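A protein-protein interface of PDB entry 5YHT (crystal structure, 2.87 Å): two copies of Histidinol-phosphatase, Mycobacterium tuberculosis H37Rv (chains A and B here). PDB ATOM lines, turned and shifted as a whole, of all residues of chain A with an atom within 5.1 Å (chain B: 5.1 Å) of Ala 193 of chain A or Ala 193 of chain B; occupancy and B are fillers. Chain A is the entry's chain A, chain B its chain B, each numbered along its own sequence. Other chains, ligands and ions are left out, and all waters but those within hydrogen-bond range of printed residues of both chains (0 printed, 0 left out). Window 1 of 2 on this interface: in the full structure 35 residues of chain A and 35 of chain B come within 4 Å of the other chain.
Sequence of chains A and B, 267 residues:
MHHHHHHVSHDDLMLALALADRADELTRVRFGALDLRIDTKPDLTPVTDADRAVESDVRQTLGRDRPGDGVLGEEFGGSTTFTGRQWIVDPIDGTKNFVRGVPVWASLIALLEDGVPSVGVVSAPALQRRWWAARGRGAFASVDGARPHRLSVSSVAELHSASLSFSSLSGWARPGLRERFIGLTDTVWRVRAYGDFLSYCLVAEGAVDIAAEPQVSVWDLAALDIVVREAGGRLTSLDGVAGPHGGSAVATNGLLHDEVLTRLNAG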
ATOM      1  N   SER A 165      -6.200 -17.162 -22.412  1.00  0.00           N
ATOM      2  CA  SER A 165      -5.104 -16.295 -21.902  1.00  0.00           C
ATOM      3  C   SER A 165      -3.759 -17.002 -21.914  1.00  0.00           C
ATOM      4  O   SER A 165      -3.652 -18.120 -21.450  1.00  0.00           O
ATOM      5  CB  SER A 165      -5.395 -15.773 -20.497  1.00  0.00           C
ATOM      6  OG  SER A 165      -4.382 -14.885 -20.056  1.00  0.00           O
ATOM      7  N   PHE A 166      -2.735 -16.364 -22.453  1.00  0.00           N
ATOM      8  CA  PHE A 166      -1.405 -16.971 -22.462  1.00  0.00           C
ATOM      9  C   PHE A 166      -0.358 -16.109 -21.749  1.00  0.00           C
ATOM     10  O   PHE A 166      -0.720 -15.273 -20.924  1.00  0.00           O
ATOM     11  CB  PHE A 166      -0.999 -17.401 -23.887  1.00  0.00           C
ATOM     12  CG  PHE A 166      -0.771 -16.268 -24.852  1.00  0.00           C
ATOM     13  CD1 PHE A 166      -1.840 -15.565 -25.398  1.00  0.00           C
ATOM     14  CD2 PHE A 166       0.512 -15.940 -25.273  1.00  0.00           C
ATOM     15  CE1 PHE A 166      -1.629 -14.520 -26.303  1.00  0.00           C
ATOM     16  CE2 PHE A 166       0.723 -14.910 -26.188  1.00  0.00           C
ATOM     17  CZ  PHE A 166      -0.344 -14.196 -26.703  1.00  0.00           C
ATOM     18  N   SER A 167       0.926 -16.332 -22.024  1.00  0.00           N
ATOM     19  CA  SER A 167       1.982 -15.477 -21.454  1.00  0.00           C
ATOM     20  C   SER A 167       2.663 -14.571 -22.479  1.00  0.00           C
ATOM     21  O   SER A 167       2.472 -13.344 -22.457  1.00  0.00           O
ATOM     22  CB  SER A 167       2.997 -16.284 -20.640  1.00  0.00           C
ATOM     23  OG  SER A 167       2.516 -16.484 -19.325  1.00  0.00           O
ATOM     24  N   SER A 168       3.452 -15.170 -23.366  1.00  0.00           N
ATOM     25  CA  SER A 168       4.123 -14.434 -24.423  1.00  0.00           C
ATOM     26  C   SER A 168       4.289 -15.362 -25.600  1.00  0.00           C
ATOM     27  O   SER A 168       4.292 -16.589 -25.429  1.00  0.00           O
ATOM     28  CB  SER A 168       5.488 -13.906 -23.958  1.00  0.00           C
ATOM     29  OG  SER A 168       6.417 -14.958 -23.754  1.00  0.00           O
ATOM     30  N   VAL A 191      -8.811 -13.395 -26.952  1.00  0.00           N
ATOM     31  CA  VAL A 191      -7.411 -13.687 -26.630  1.00  0.00           C
ATOM     32  C   VAL A 191      -6.844 -12.556 -25.787  1.00  0.00           C
ATOM     33  O   VAL A 191      -6.909 -11.387 -26.171  1.00  0.00           O
ATOM     34  CB  VAL A 191      -6.533 -13.879 -27.898  1.00  0.00           C
ATOM     35  CG1 VAL A 191      -5.065 -14.002 -27.537  1.00  0.00           C
ATOM     36  CG2 VAL A 191      -6.938 -15.115 -28.674  1.00  0.00           C
ATOM     37  N   ARG A 192      -6.319 -12.915 -24.622  1.00  0.00           N
ATOM     38  CA  ARG A 192      -5.438 -12.033 -23.847  1.00  0.00           C
ATOM     39  C   ARG A 192      -4.193 -12.795 -23.375  1.00  0.00           C
ATOM     40  O   ARG A 192      -4.070 -13.998 -23.614  1.00  0.00           O
ATOM     41  CB  ARG A 192      -6.183 -11.416 -22.664  1.00  0.00           C
ATOM     42  CG  ARG A 192      -7.225 -10.382 -23.040  1.00  0.00           C
ATOM     43  CD  ARG A 192      -6.558  -9.092 -23.443  1.00  0.00           C
ATOM     44  NE  ARG A 192      -7.492  -8.006 -23.743  1.00  0.00           N
ATOM     45  CZ  ARG A 192      -8.031  -7.799 -24.943  1.00  0.00           C
ATOM     46  NH1 ARG A 192      -7.801  -8.635 -25.955  1.00  0.00           N
ATOM     47  NH2 ARG A 192      -8.823  -6.758 -25.124  1.00  0.00           N
ATOM     48  N   ALA A 193      -3.257 -12.094 -22.739  1.00  0.00           N
ATOM     49  CA  ALA A 193      -2.116 -12.754 -22.138  1.00  0.00           C
ATOM     50  C   ALA A 193      -1.868 -12.138 -20.794  1.00  0.00           C
ATOM     51  O   ALA A 193      -0.997 -11.291 -20.653  1.00  0.00           O
ATOM     52  CB  ALA A 193      -0.897 -12.635 -23.033  1.00  0.00           C
ATOM     53  N   TYR A 194      -2.665 -12.523 -19.805  1.00  0.00           N
ATOM     54  CA  TYR A 194      -2.527 -11.931 -18.471  1.00  0.00           C
ATOM     55  C   TYR A 194      -1.269 -12.438 -17.803  1.00  0.00           C
ATOM     56  O   TYR A 194      -0.715 -11.789 -16.931  1.00  0.00           O
ATOM     57  CB  TYR A 194      -3.749 -12.216 -17.605  1.00  0.00           C
ATOM     58  CG  TYR A 194      -5.022 -11.648 -18.188  1.00  0.00           C
ATOM     59  CD1 TYR A 194      -5.320 -10.277 -18.080  1.00  0.00           C
ATOM     60  CD2 TYR A 194      -5.922 -12.472 -18.870  1.00  0.00           C
ATOM     61  CE1 TYR A 194      -6.480  -9.753 -18.627  1.00  0.00           C
ATOM     62  CE2 TYR A 194      -7.081 -11.957 -19.413  1.00  0.00           C
ATOM     63  CZ  TYR A 194      -7.349 -10.612 -19.290  1.00  0.00           C
ATOM     64  OH  TYR A 194      -8.505 -10.171 -19.835  1.00  0.00           O
ATOM     65  N   GLY A 195      -0.828 -13.609 -18.243  1.00  0.00           N
ATOM     66  CA  GLY A 195       0.477 -14.124 -17.903  1.00  0.00           C
ATOM     67  C   GLY A 195       0.561 -14.933 -16.620  1.00  0.00           C
ATOM     68  O   GLY A 195      -0.230 -14.750 -15.673  1.00  0.00           O
ATOM     69  N   SER B 165       3.050  -4.197 -23.827  1.00  0.00           N
ATOM     70  CA  SER B 165       1.711  -4.794 -23.634  1.00  0.00           C
ATOM     71  C   SER B 165       0.743  -4.483 -24.803  1.00  0.00           C
ATOM     72  O   SER B 165       0.631  -3.340 -25.282  1.00  0.00           O
ATOM     73  CB  SER B 165       1.116  -4.373 -22.299  1.00  0.00           C
ATOM     74  OG  SER B 165      -0.172  -4.930 -22.107  1.00  0.00           O
ATOM     75  N   PHE B 166       0.071  -5.508 -25.298  1.00  0.00           N
ATOM     76  CA  PHE B 166      -0.893  -5.293 -26.373  1.00  0.00           C
ATOM     77  C   PHE B 166      -2.277  -5.830 -25.990  1.00  0.00           C
ATOM     78  O   PHE B 166      -2.577  -5.996 -24.799  1.00  0.00           O
ATOM     79  CB  PHE B 166      -0.373  -5.808 -27.732  1.00  0.00           C
ATOM     80  CG  PHE B 166      -0.186  -7.307 -27.809  1.00  0.00           C
ATOM     81  CD1 PHE B 166       0.858  -7.946 -27.133  1.00  0.00           C
ATOM     82  CD2 PHE B 166      -1.036  -8.075 -28.593  1.00  0.00           C
ATOM     83  CE1 PHE B 166       1.016  -9.314 -27.216  1.00  0.00           C
ATOM     84  CE2 PHE B 166      -0.875  -9.450 -28.682  1.00  0.00           C
ATOM     85  CZ  PHE B 166       0.149 -10.072 -27.994  1.00  0.00           C
ATOM     86  N   SER B 167      -3.125  -6.056 -26.987  1.00  0.00           N
ATOM     87  CA  SER B 167      -4.454  -6.565 -26.733  1.00  0.00           C
ATOM     88  C   SER B 167      -4.638  -7.994 -27.200  1.00  0.00           C
ATOM     89  O   SER B 167      -4.792  -8.886 -26.369  1.00  0.00           O
ATOM     90  CB  SER B 167      -5.520  -5.620 -27.271  1.00  0.00           C
ATOM     91  OG  SER B 167      -5.776  -4.621 -26.288  1.00  0.00           O
ATOM     92  N   SER B 168      -4.625  -8.207 -28.512  1.00  0.00           N
ATOM     93  CA  SER B 168      -4.726  -9.546 -29.084  1.00  0.00           C
ATOM     94  C   SER B 168      -4.034  -9.504 -30.421  1.00  0.00           C
ATOM     95  O   SER B 168      -3.771  -8.420 -30.945  1.00  0.00           O
ATOM     96  CB  SER B 168      -6.192  -9.976 -29.241  1.00  0.00           C
ATOM     97  OG  SER B 168      -6.836  -9.264 -30.286  1.00  0.00           O
ATOM     98  N   VAL B 191       6.960  -9.237 -23.102  1.00  0.00           N
ATOM     99  CA  VAL B 191       5.686  -9.098 -23.810  1.00  0.00           C
ATOM    100  C   VAL B 191       4.567  -9.652 -22.955  1.00  0.00           C
ATOM    101  O   VAL B 191       4.635 -10.787 -22.483  1.00  0.00           O
ATOM    102  CB  VAL B 191       5.682  -9.846 -25.144  1.00  0.00           C
ATOM    103  CG1 VAL B 191       4.320  -9.742 -25.806  1.00  0.00           C
ATOM    104  CG2 VAL B 191       6.739  -9.287 -26.070  1.00  0.00           C
ATOM    105  N   ARG B 192       3.558  -8.819 -22.725  1.00  0.00           N
ATOM    106  CA  ARG B 192       2.251  -9.266 -22.235  1.00  0.00           C
ATOM    107  C   ARG B 192       1.122  -8.681 -23.077  1.00  0.00           C
ATOM    108  O   ARG B 192       1.355  -7.922 -24.027  1.00  0.00           O
ATOM    109  CB  ARG B 192       2.066  -8.946 -20.747  1.00  0.00           C
ATOM    110  CG  ARG B 192       2.896  -9.830 -19.815  1.00  0.00           C
ATOM    111  CD  ARG B 192       2.374 -11.264 -19.745  1.00  0.00           C
ATOM    112  NE  ARG B 192       3.090 -12.094 -18.772  1.00  0.00           N
ATOM    113  CZ  ARG B 192       4.200 -12.787 -19.045  1.00  0.00           C
ATOM    114  NH1 ARG B 192       4.744 -12.750 -20.262  1.00  0.00           N
ATOM    115  NH2 ARG B 192       4.776 -13.515 -18.100  1.00  0.00           N
ATOM    116  N   ALA B 193      -0.101  -9.090 -22.775  1.00  0.00           N
ATOM    117  CA  ALA B 193      -1.260  -8.441 -23.354  1.00  0.00           C
ATOM    118  C   ALA B 193      -2.315  -8.214 -22.263  1.00  0.00           C
ATOM    119  O   ALA B 193      -3.261  -8.994 -22.125  1.00  0.00           O
ATOM    120  CB  ALA B 193      -1.790  -9.253 -24.523  1.00  0.00           C
ATOM    121  N   TYR B 194      -2.121  -7.166 -21.459  1.00  0.00           N
ATOM    122  CA  TYR B 194      -3.056  -6.839 -20.385  1.00  0.00           C
ATOM    123  C   TYR B 194      -4.359  -6.312 -20.960  1.00  0.00           C
ATOM    124  O   TYR B 194      -5.416  -6.438 -20.330  1.00  0.00           O
ATOM    125  CB  TYR B 194      -2.443  -5.842 -19.408  1.00  0.00           C
ATOM    126  CG  TYR B 194      -1.236  -6.403 -18.740  1.00  0.00           C
ATOM    127  CD1 TYR B 194      -1.344  -7.478 -17.858  1.00  0.00           C
ATOM    128  CD2 TYR B 194       0.029  -5.902 -19.025  1.00  0.00           C
ATOM    129  CE1 TYR B 194      -0.224  -8.035 -17.271  1.00  0.00           C
ATOM    130  CE2 TYR B 194       1.150  -6.445 -18.436  1.00  0.00           C
ATOM    131  CZ  TYR B 194       1.017  -7.516 -17.566  1.00  0.00           C
ATOM    132  OH  TYR B 194       2.120  -8.073 -16.972  1.00  0.00           O
ATOM    133  N   GLY B 195      -4.256  -5.729 -22.162  1.00  0.00           N
ATOM    134  CA  GLY B 195      -5.399  -5.402 -23.000  1.00  0.00           C
ATOM    135  C   GLY B 195      -6.054  -4.066 -22.728  1.00  0.00           C
ATOM    136  O   GLY B 195      -6.006  -3.541 -21.600  1.00  0.00           O
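Of chain B, only Arg 192 and Ala 193 come within 4 Å of Ala 193 of chain A.
Printed residues of chain A within 4 Å of Ser 168 of chain B: Val 191 and Arg 192.
Printed residues of chain A within 4 Å of Gly 195 of chain B: Arg 192.
Printed residues of chain B within 4 Å of Gly 195 of chain A: Arg 192.
Printed residues of chain B within 4 Å of Ser 168 of chain A: Val 191 and Arg 192.
Phe 166 of chain A touches none of the printed residues of chain B.
The nearest residue of chain B that does not touch Ala 193 of chain A is Tyr 194 of chain B (4.4 Å).
Among the printed residues, merely in contact across the chains: Gly 195 of chain A with Arg 192 of chain B, Arg 192 of chain A with Gly 195 of chain B, Val 191 of chain A with Ser 168 of chain B, Ala 193 of chain A with Arg 192 of chain B, Arg 192 of chain A with Ala 193 of chain B, Ser 168 of chain A with Val 191 of chain B, Tyr 194 of chain A with Tyr 194 of chain B, Arg 192 of chain A with Ser 168 of chain B and Ser 168 of chain A with Arg 192 of chain B.
The backbone carbonyl oxygen (O) of Val 191 of chain B lies close to the backbone carbonyl oxygen (O) of Ser 167 of chain A (3.3 Å).
The backbone NH of Ala 193 of chain A lies within hydrogen-bond range of the backbone carbonyl oxygen of Ala 193 of chain B.
The backbone carbonyl oxygen of Ser 167 of chain A is in hydrogen-bond range of the guanidinium group of Arg 192 of chain B (3.2 Å).
The backbone carbonyl oxygen of Val 191 of chain A sits close to the backbone carbonyl oxygen of Ser 167 of chain B, at 3.3 Å.
NH1 of Arg 192 of chain A lies within hydrogen-bond range of O of Ser 167 of chain B.
Hydrophobic or aromatic side chains of chain B within 4 Å of the printed part of chain A: Ala 193 and Tyr 194.
Of the 9 printed residues of chain A, 7 touch a printed residue of chain B.
Hydrophobic or aromatic side chains of chain A within 4 Å of the printed part of chain B: Ala 193 and Tyr 194.
The backbone carbonyl oxygen of Phe 166 of chain A lies within hydrogen-bond range of the backbone NH of Gly 195 of chain A (3.2 Å).
The backbone carbonyl oxygen of Phe 166 of chain B lies within hydrogen-bond range of the backbone NH of Gly 195 of chain B (3.1 Å).
The backbone NH of Phe 166 of chain A sits at hydrogen-bond distance from the backbone carbonyl oxygen of Arg 192 of chain A (3.0 Å).
The backbone NH (N) of Tyr 194 of chain B lies within hydrogen-bond range of the side-chain hydroxyl (OG) of Ser 165 of chain B (3.0 Å).
N of Phe 166 of chain B lies within hydrogen-bond range of O of Arg 192 of chain B (3.0 Å).
The backbone NH (N) of Tyr 194 of chain A sits at hydrogen-bond distance from the side-chain hydroxyl (OG) of Ser 165 of chain A, 2.9 Å away.
Ser 167 of chain A touches Val 191 of chain B, and with the chains exchanged Val 191 of chain A touches Ser 167 of chain B.
Ser 168 of chain A touches Arg 192 of chain B, and with the chains exchanged Arg 192 of chain A touches Ser 168 of chain B.
Arg 192 of chain A touches Gly 195 of chain B, and with the chains exchanged Gly 195 of chain A touches Arg 192 of chain B.
Ala 193 of chain B touches its own counterpart, Ala 193 of chain A.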
